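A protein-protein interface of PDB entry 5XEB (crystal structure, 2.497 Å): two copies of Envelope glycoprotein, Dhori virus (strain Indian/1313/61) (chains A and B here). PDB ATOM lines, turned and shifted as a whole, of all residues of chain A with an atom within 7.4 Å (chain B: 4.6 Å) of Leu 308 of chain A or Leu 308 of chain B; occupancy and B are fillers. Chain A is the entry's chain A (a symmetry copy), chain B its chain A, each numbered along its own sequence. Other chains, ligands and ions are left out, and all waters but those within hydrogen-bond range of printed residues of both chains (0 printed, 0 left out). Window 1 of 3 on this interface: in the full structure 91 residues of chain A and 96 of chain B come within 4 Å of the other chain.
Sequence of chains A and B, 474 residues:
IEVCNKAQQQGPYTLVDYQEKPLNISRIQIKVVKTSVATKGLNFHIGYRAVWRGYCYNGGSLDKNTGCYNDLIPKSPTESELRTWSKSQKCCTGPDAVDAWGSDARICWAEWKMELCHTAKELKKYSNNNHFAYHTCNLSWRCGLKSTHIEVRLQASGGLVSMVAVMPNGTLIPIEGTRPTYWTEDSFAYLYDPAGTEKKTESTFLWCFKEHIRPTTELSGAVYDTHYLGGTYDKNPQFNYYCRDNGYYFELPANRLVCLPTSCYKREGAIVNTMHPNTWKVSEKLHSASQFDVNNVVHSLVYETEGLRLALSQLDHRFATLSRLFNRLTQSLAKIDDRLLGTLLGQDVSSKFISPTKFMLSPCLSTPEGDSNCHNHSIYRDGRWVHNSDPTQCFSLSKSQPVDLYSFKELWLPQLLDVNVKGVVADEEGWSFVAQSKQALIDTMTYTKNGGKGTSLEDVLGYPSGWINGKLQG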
ATOM      1  N   LEU A 301       7.439 -31.946 -16.659  1.00  0.00           N
ATOM      2  CA  LEU A 301       6.817 -30.638 -16.492  1.00  0.00           C
ATOM      3  C   LEU A 301       7.256 -29.983 -15.187  1.00  0.00           C
ATOM      4  O   LEU A 301       7.487 -28.770 -15.144  1.00  0.00           O
ATOM      5  CB  LEU A 301       5.296 -30.771 -16.545  1.00  0.00           C
ATOM      6  CG  LEU A 301       4.482 -29.485 -16.392  1.00  0.00           C
ATOM      7  CD1 LEU A 301       4.822 -28.501 -17.501  1.00  0.00           C
ATOM      8  CD2 LEU A 301       2.993 -29.798 -16.383  1.00  0.00           C
ATOM      9  N   VAL A 302       7.400 -30.773 -14.120  1.00  0.00           N
ATOM     10  CA  VAL A 302       7.822 -30.220 -12.832  1.00  0.00           C
ATOM     11  C   VAL A 302       9.252 -29.696 -12.916  1.00  0.00           C
ATOM     12  O   VAL A 302       9.546 -28.576 -12.483  1.00  0.00           O
ATOM     13  CB  VAL A 302       7.671 -31.273 -11.721  1.00  0.00           C
ATOM     14  CG1 VAL A 302       8.332 -30.789 -10.440  1.00  0.00           C
ATOM     15  CG2 VAL A 302       6.203 -31.582 -11.483  1.00  0.00           C
ATOM     16  N   TYR A 303      10.162 -30.509 -13.457  1.00  0.00           N
ATOM     17  CA  TYR A 303      11.547 -30.085 -13.661  1.00  0.00           C
ATOM     18  C   TYR A 303      11.610 -28.787 -14.464  1.00  0.00           C
ATOM     19  O   TYR A 303      12.289 -27.820 -14.079  1.00  0.00           O
ATOM     20  CB  TYR A 303      12.296 -31.216 -14.374  1.00  0.00           C
ATOM     21  CG  TYR A 303      13.797 -31.081 -14.466  1.00  0.00           C
ATOM     22  CD1 TYR A 303      14.608 -31.385 -13.382  1.00  0.00           C
ATOM     23  CD2 TYR A 303      14.406 -30.699 -15.653  1.00  0.00           C
ATOM     24  CE1 TYR A 303      15.984 -31.282 -13.470  1.00  0.00           C
ATOM     25  CE2 TYR A 303      15.780 -30.593 -15.751  1.00  0.00           C
ATOM     26  CZ  TYR A 303      16.564 -30.886 -14.656  1.00  0.00           C
ATOM     27  OH  TYR A 303      17.934 -30.784 -14.746  1.00  0.00           O
ATOM     28  N   GLU A 304      10.879 -28.753 -15.579  1.00  0.00           N
ATOM     29  CA  GLU A 304      10.814 -27.562 -16.419  1.00  0.00           C
ATOM     30  C   GLU A 304      10.354 -26.345 -15.625  1.00  0.00           C
ATOM     31  O   GLU A 304      11.011 -25.295 -15.634  1.00  0.00           O
ATOM     32  CB  GLU A 304       9.874 -27.830 -17.593  1.00  0.00           C
ATOM     33  CG  GLU A 304       9.671 -26.658 -18.514  1.00  0.00           C
ATOM     34  CD  GLU A 304      10.899 -26.358 -19.337  1.00  0.00           C
ATOM     35  OE1 GLU A 304      11.809 -27.213 -19.400  1.00  0.00           O
ATOM     36  OE2 GLU A 304      10.947 -25.261 -19.926  1.00  0.00           O
ATOM     37  N   THR A 305       9.222 -26.466 -14.926  1.00  0.00           N
ATOM     38  CA  THR A 305       8.699 -25.334 -14.171  1.00  0.00           C
ATOM     39  C   THR A 305       9.653 -24.905 -13.066  1.00  0.00           C
ATOM     40  O   THR A 305       9.657 -23.734 -12.680  1.00  0.00           O
ATOM     41  CB  THR A 305       7.331 -25.671 -13.578  1.00  0.00           C
ATOM     42  OG1 THR A 305       7.458 -26.800 -12.708  1.00  0.00           O
ATOM     43  CG2 THR A 305       6.338 -25.990 -14.684  1.00  0.00           C
ATOM     44  N   GLU A 306      10.458 -25.829 -12.540  1.00  0.00           N
ATOM     45  CA  GLU A 306      11.511 -25.433 -11.610  1.00  0.00           C
ATOM     46  C   GLU A 306      12.526 -24.531 -12.301  1.00  0.00           C
ATOM     47  O   GLU A 306      12.906 -23.479 -11.769  1.00  0.00           O
ATOM     48  CB  GLU A 306      12.191 -26.668 -11.020  1.00  0.00           C
ATOM     49  CG  GLU A 306      11.400 -27.323  -9.902  1.00  0.00           C
ATOM     50  CD  GLU A 306      11.378 -26.480  -8.644  1.00  0.00           C
ATOM     51  OE1 GLU A 306      12.450 -25.986  -8.238  1.00  0.00           O
ATOM     52  OE2 GLU A 306      10.286 -26.304  -8.062  1.00  0.00           O
ATOM     53  N   GLY A 307      12.969 -24.923 -13.500  1.00  0.00           N
ATOM     54  CA  GLY A 307      13.837 -24.040 -14.267  1.00  0.00           C
ATOM     55  C   GLY A 307      13.223 -22.670 -14.500  1.00  0.00           C
ATOM     56  O   GLY A 307      13.896 -21.641 -14.368  1.00  0.00           O
ATOM     57  N   LEU A 308      11.928 -22.638 -14.829  1.00  0.00           N
ATOM     58  CA  LEU A 308      11.255 -21.366 -15.089  1.00  0.00           C
ATOM     59  C   LEU A 308      11.163 -20.514 -13.827  1.00  0.00           C
ATOM     60  O   LEU A 308      11.334 -19.291 -13.886  1.00  0.00           O
ATOM     61  CB  LEU A 308       9.866 -21.624 -15.671  1.00  0.00           C
ATOM     62  CG  LEU A 308       9.726 -21.789 -17.189  1.00  0.00           C
ATOM     63  CD1 LEU A 308      11.062 -22.049 -17.862  1.00  0.00           C
ATOM     64  CD2 LEU A 308       8.726 -22.886 -17.527  1.00  0.00           C
ATOM     65  N   ARG A 309      10.884 -21.142 -12.680  1.00  0.00           N
ATOM     66  CA  ARG A 309      10.893 -20.422 -11.410  1.00  0.00           C
ATOM     67  C   ARG A 309      12.259 -19.811 -11.140  1.00  0.00           C
ATOM     68  O   ARG A 309      12.361 -18.652 -10.714  1.00  0.00           O
ATOM     69  CB  ARG A 309      10.506 -21.362 -10.269  1.00  0.00           C
ATOM     70  CG  ARG A 309       9.078 -21.859 -10.312  1.00  0.00           C
ATOM     71  CD  ARG A 309       8.878 -23.002  -9.327  1.00  0.00           C
ATOM     72  NE  ARG A 309       9.104 -22.580  -7.950  1.00  0.00           N
ATOM     73  CZ  ARG A 309       8.179 -22.008  -7.184  1.00  0.00           C
ATOM     74  NH1 ARG A 309       6.962 -21.788  -7.665  1.00  0.00           N
ATOM     75  NH2 ARG A 309       8.472 -21.654  -5.940  1.00  0.00           N
ATOM     76  N   LEU A 310      13.323 -20.582 -11.377  1.00  0.00           N
ATOM     77  CA  LEU A 310      14.674 -20.063 -11.194  1.00  0.00           C
ATOM     78  C   LEU A 310      14.911 -18.832 -12.064  1.00  0.00           C
ATOM     79  O   LEU A 310      15.291 -17.767 -11.560  1.00  0.00           O
ATOM     80  CB  LEU A 310      15.693 -21.156 -11.510  1.00  0.00           C
ATOM     81  CG  LEU A 310      17.160 -20.726 -11.555  1.00  0.00           C
ATOM     82  CD1 LEU A 310      17.616 -20.249 -10.188  1.00  0.00           C
ATOM     83  CD2 LEU A 310      18.033 -21.865 -12.052  1.00  0.00           C
ATOM     84  N   ALA A 311      14.674 -18.958 -13.374  1.00  0.00           N
ATOM     85  CA  ALA A 311      14.954 -17.851 -14.287  1.00  0.00           C
ATOM     86  C   ALA A 311      14.127 -16.616 -13.937  1.00  0.00           C
ATOM     87  O   ALA A 311      14.663 -15.504 -13.825  1.00  0.00           O
ATOM     88  CB  ALA A 311      14.695 -18.285 -15.729  1.00  0.00           C
ATOM     89  N   LEU A 312      12.815 -16.798 -13.754  1.00  0.00           N
ATOM     90  CA  LEU A 312      11.945 -15.664 -13.453  1.00  0.00           C
ATOM     91  C   LEU A 312      12.346 -14.983 -12.149  1.00  0.00           C
ATOM     92  O   LEU A 312      12.328 -13.749 -12.055  1.00  0.00           O
ATOM     93  CB  LEU A 312      10.487 -16.123 -13.396  1.00  0.00           C
ATOM     94  CG  LEU A 312       9.836 -16.490 -14.734  1.00  0.00           C
ATOM     95  CD1 LEU A 312       8.448 -17.063 -14.516  1.00  0.00           C
ATOM     96  CD2 LEU A 312       9.774 -15.278 -15.647  1.00  0.00           C
ATOM     97  N   SER A 313      12.715 -15.769 -11.133  1.00  0.00           N
ATOM     98  CA  SER A 313      13.156 -15.175  -9.875  1.00  0.00           C
ATOM     99  C   SER A 313      14.453 -14.398 -10.059  1.00  0.00           C
ATOM    100  O   SER A 313      14.639 -13.333  -9.456  1.00  0.00           O
ATOM    101  CB  SER A 313      13.324 -16.260  -8.812  1.00  0.00           C
ATOM    102  OG  SER A 313      14.284 -17.221  -9.215  1.00  0.00           O
ATOM    103  N   GLN A 314      15.361 -14.910 -10.894  1.00  0.00           N
ATOM    104  CA  GLN A 314      16.600 -14.188 -11.169  1.00  0.00           C
ATOM    105  C   GLN A 314      16.317 -12.840 -11.821  1.00  0.00           C
ATOM    106  O   GLN A 314      16.875 -11.811 -11.417  1.00  0.00           O
ATOM    107  CB  GLN A 314      17.518 -15.038 -12.048  1.00  0.00           C
ATOM    108  CG  GLN A 314      18.134 -16.226 -11.328  1.00  0.00           C
ATOM    109  CD  GLN A 314      19.001 -17.071 -12.236  1.00  0.00           C
ATOM    110  OE1 GLN A 314      18.743 -17.184 -13.435  1.00  0.00           O
ATOM    111  NE2 GLN A 314      20.043 -17.668 -11.670  1.00  0.00           N
ATOM    112  N   LEU A 413       4.618 -13.664 -25.996  1.00  0.00           N
ATOM    113  CA  LEU A 413       3.951 -14.365 -24.908  1.00  0.00           C
ATOM    114  C   LEU A 413       3.480 -15.728 -25.392  1.00  0.00           C
ATOM    115  O   LEU A 413       2.815 -15.812 -26.431  1.00  0.00           O
ATOM    116  CB  LEU A 413       2.768 -13.563 -24.385  1.00  0.00           C
ATOM    117  CG  LEU A 413       3.016 -12.692 -23.150  1.00  0.00           C
ATOM    118  CD1 LEU A 413       4.313 -11.909 -23.271  1.00  0.00           C
ATOM    119  CD2 LEU A 413       1.838 -11.758 -22.899  1.00  0.00           C
ATOM    120  N   PRO A 414       3.804 -16.802 -24.677  1.00  0.00           N
ATOM    121  CA  PRO A 414       3.434 -18.141 -25.150  1.00  0.00           C
ATOM    122  C   PRO A 414       1.925 -18.315 -25.188  1.00  0.00           C
ATOM    123  O   PRO A 414       1.210 -17.899 -24.275  1.00  0.00           O
ATOM    124  CB  PRO A 414       4.080 -19.065 -24.116  1.00  0.00           C
ATOM    125  CG  PRO A 414       4.118 -18.234 -22.870  1.00  0.00           C
ATOM    126  CD  PRO A 414       4.435 -16.843 -23.347  1.00  0.00           C
ATOM    127  N   GLU B 304      -0.525 -23.568 -16.328  1.00  0.00           N
ATOM    128  CA  GLU B 304       0.873 -23.177 -16.182  1.00  0.00           C
ATOM    129  C   GLU B 304       1.243 -22.062 -17.153  1.00  0.00           C
ATOM    130  O   GLU B 304       1.778 -21.021 -16.751  1.00  0.00           O
ATOM    131  CB  GLU B 304       1.759 -24.402 -16.399  1.00  0.00           C
ATOM    132  CG  GLU B 304       3.236 -24.127 -16.331  1.00  0.00           C
ATOM    133  CD  GLU B 304       3.698 -23.822 -14.928  1.00  0.00           C
ATOM    134  OE1 GLU B 304       2.939 -24.088 -13.970  1.00  0.00           O
ATOM    135  OE2 GLU B 304       4.828 -23.317 -14.787  1.00  0.00           O
ATOM    136  N   THR B 305       0.962 -22.262 -18.445  1.00  0.00           N
ATOM    137  CA  THR B 305       1.320 -21.257 -19.440  1.00  0.00           C
ATOM    138  C   THR B 305       0.586 -19.945 -19.204  1.00  0.00           C
ATOM    139  O   THR B 305       1.092 -18.884 -19.573  1.00  0.00           O
ATOM    140  CB  THR B 305       1.032 -21.771 -20.848  1.00  0.00           C
ATOM    141  OG1 THR B 305      -0.361 -22.075 -20.966  1.00  0.00           O
ATOM    142  CG2 THR B 305       1.850 -23.020 -21.136  1.00  0.00           C
ATOM    143  N   GLU B 306      -0.604 -19.993 -18.603  1.00  0.00           N
ATOM    144  CA  GLU B 306      -1.264 -18.757 -18.195  1.00  0.00           C
ATOM    145  C   GLU B 306      -0.441 -18.035 -17.136  1.00  0.00           C
ATOM    146  O   GLU B 306      -0.212 -16.821 -17.229  1.00  0.00           O
ATOM    147  CB  GLU B 306      -2.674 -19.052 -17.683  1.00  0.00           C
ATOM    148  CG  GLU B 306      -3.690 -19.270 -18.789  1.00  0.00           C
ATOM    149  CD  GLU B 306      -4.006 -17.993 -19.540  1.00  0.00           C
ATOM    150  OE1 GLU B 306      -4.238 -16.958 -18.882  1.00  0.00           O
ATOM    151  OE2 GLU B 306      -4.017 -18.022 -20.789  1.00  0.00           O
ATOM    152  N   GLY B 307       0.027 -18.771 -16.123  1.00  0.00           N
ATOM    153  CA  GLY B 307       0.928 -18.165 -15.153  1.00  0.00           C
ATOM    154  C   GLY B 307       2.160 -17.554 -15.798  1.00  0.00           C
ATOM    155  O   GLY B 307       2.578 -16.445 -15.445  1.00  0.00           O
ATOM    156  N   LEU B 308       2.745 -18.261 -16.770  1.00  0.00           N
ATOM    157  CA  LEU B 308       3.945 -17.761 -17.438  1.00  0.00           C
ATOM    158  C   LEU B 308       3.651 -16.505 -18.252  1.00  0.00           C
ATOM    159  O   LEU B 308       4.462 -15.572 -18.276  1.00  0.00           O
ATOM    160  CB  LEU B 308       4.539 -18.855 -18.325  1.00  0.00           C
ATOM    161  CG  LEU B 308       5.530 -19.846 -17.702  1.00  0.00           C
ATOM    162  CD1 LEU B 308       5.486 -19.823 -16.184  1.00  0.00           C
ATOM    163  CD2 LEU B 308       5.294 -21.254 -18.230  1.00  0.00           C
ATOM    164  N   ARG B 309       2.500 -16.470 -18.932  1.00  0.00           N
ATOM    165  CA  ARG B 309       2.086 -15.262 -19.641  1.00  0.00           C
ATOM    166  C   ARG B 309       1.952 -14.088 -18.684  1.00  0.00           C
ATOM    167  O   ARG B 309       2.397 -12.972 -18.985  1.00  0.00           O
ATOM    168  CB  ARG B 309       0.760 -15.503 -20.361  1.00  0.00           C
ATOM    169  CG  ARG B 309       0.827 -16.500 -21.498  1.00  0.00           C
ATOM    170  CD  ARG B 309      -0.573 -16.893 -21.950  1.00  0.00           C
ATOM    171  NE  ARG B 309      -1.316 -15.753 -22.473  1.00  0.00           N
ATOM    172  CZ  ARG B 309      -1.235 -15.323 -23.728  1.00  0.00           C
ATOM    173  NH1 ARG B 309      -0.439 -15.940 -24.592  1.00  0.00           N
ATOM    174  NH2 ARG B 309      -1.947 -14.275 -24.120  1.00  0.00           N
ATOM    175  N   LEU B 310       1.332 -14.321 -17.525  1.00  0.00           N
ATOM    176  CA  LEU B 310       1.203 -13.266 -16.526  1.00  0.00           C
ATOM    177  C   LEU B 310       2.569 -12.733 -16.111  1.00  0.00           C
ATOM    178  O   LEU B 310       2.827 -11.525 -16.192  1.00  0.00           O
ATOM    179  CB  LEU B 310       0.435 -13.796 -15.315  1.00  0.00           C
ATOM    180  CG  LEU B 310       0.375 -12.878 -14.093  1.00  0.00           C
ATOM    181  CD1 LEU B 310      -0.383 -11.605 -14.421  1.00  0.00           C
ATOM    182  CD2 LEU B 310      -0.258 -13.601 -12.916  1.00  0.00           C
ATOM    183  N   ALA B 311       3.466 -13.625 -15.677  1.00  0.00           N
ATOM    184  CA  ALA B 311       4.770 -13.186 -15.184  1.00  0.00           C
ATOM    185  C   ALA B 311       5.558 -12.454 -16.266  1.00  0.00           C
ATOM    186  O   ALA B 311       6.081 -11.353 -16.037  1.00  0.00           O
ATOM    187  CB  ALA B 311       5.559 -14.384 -14.657  1.00  0.00           C
ATOM    188  N   LEU B 312       5.646 -13.050 -17.460  1.00  0.00           N
ATOM    189  CA  LEU B 312       6.412 -12.435 -18.541  1.00  0.00           C
ATOM    190  C   LEU B 312       5.848 -11.071 -18.920  1.00  0.00           C
ATOM    191  O   LEU B 312       6.607 -10.128 -19.181  1.00  0.00           O
ATOM    192  CB  LEU B 312       6.442 -13.364 -19.755  1.00  0.00           C
ATOM    193  CG  LEU B 312       7.303 -14.624 -19.629  1.00  0.00           C
ATOM    194  CD1 LEU B 312       7.126 -15.519 -20.841  1.00  0.00           C
ATOM    195  CD2 LEU B 312       8.766 -14.255 -19.449  1.00  0.00           C
ATOM    196  N   PRO B 414      15.619 -22.746 -20.112  1.00  0.00           N
ATOM    197  CA  PRO B 414      15.156 -24.133 -19.991  1.00  0.00           C
ATOM    198  C   PRO B 414      15.455 -24.926 -21.252  1.00  0.00           C
ATOM    199  O   PRO B 414      15.274 -24.441 -22.370  1.00  0.00           O
ATOM    200  CB  PRO B 414      13.651 -23.978 -19.769  1.00  0.00           C
ATOM    201  CG  PRO B 414      13.319 -22.690 -20.459  1.00  0.00           C
ATOM    202  CD  PRO B 414      14.497 -21.795 -20.185  1.00  0.00           C
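Leu 308 of chain A touches just these residues of chain B: Leu 308 and Pro 414.
Printed residues of chain B within 4 Å of Pro 414 of chain A: Arg 309 (2.6 Å) and Leu 312 (3.9 Å).
Of the printed residues of chain A, Glu 304 of chain B touches Thr 305.
No residue of chain A comes within 4 Å of Gly 307 of chain B.
Leu 308 of chain B touches one residue of chain A.
Of the printed residues of chain A, Arg 309 of chain B touches Leu 413 and Pro 414.
The nearest printed residue of chain B that does not touch Leu 308 of chain A is Glu 304 of chain B (4.8 Å).
The nearest residue of chain A that does not touch Leu 308 of chain B is Leu 312 of chain A (4.4 Å).
Among the printed residues, merely in contact across the chains: Glu 304 of chain A with Pro 414 of chain B, Thr 305 of chain A with Glu 304 of chain B, Leu 308 of chain A with Pro 414 of chain B, Leu 413 of chain A with Arg 309 of chain B, Leu 308 of chain A with Leu 308 of chain B, Pro 414 of chain A with Leu 312 of chain B and Leu 312 of chain A with Ala 311 of chain B.
The backbone carbonyl oxygen (O) of Pro 414 of chain A is in hydrogen-bond range of the guanidinium group (NH1) of Arg 309 of chain B.
Hydrophobic or aromatic side chains of chain B that line the printed part of chain A: Leu 308, Ala 311, Leu 312 and Pro 414.
Of the 16 printed residues of chain A, 6 touch a printed residue of chain B.
Printed residues of chain A that touch a printed residue of chain B: Glu 304, Thr 305, Leu 308, Leu 312, Leu 413 and Pro 414.
Among the printed residues, 8 pairs touch across the chains.
Among the printed residues, no Asp or Glu carboxylate lies within 4 Å of a Lys or Arg side-chain nitrogen of the other chain.
Glu 304 of chain A touches Pro 414 of chain B, but with the chains exchanged Pro 414 of chain A does not touch Glu 304 of chain B (7.1 Å).
Leu 308 of chain B touches its own counterpart, Leu 308 of chain A.
Leu 308 of chain A touches Pro 414 of chain B, but with the chains exchanged Pro 414 of chain A does not touch Leu 308 of chain B (4.6 Å).
Leu 312 of chain A touches Ala 311 of chain B, but with the chains exchanged Ala 311 of chain A does not touch Leu 312 of chain B (8.0 Å).
Positions printed for both chains: 304, 305, 306, 307, 308, 309, 310, 311, 312 and 414.
Of the 8 pairs that touch across the chains among the printed residues, 1 has its exchanged pair printed and touching as well.
O of Leu 301 of chain A sits close to OG1 of Thr 305 of chain A.
The side-chain carboxylate (OE2) of Glu 306 of chain B is in salt-bridge range of the guanidinium group (NE) of Arg 309 of chain B (3.9 Å).
O of Val 302 of chain A lies within hydrogen-bond range of OG1 of Thr 305 of chain A (2.8 Å).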
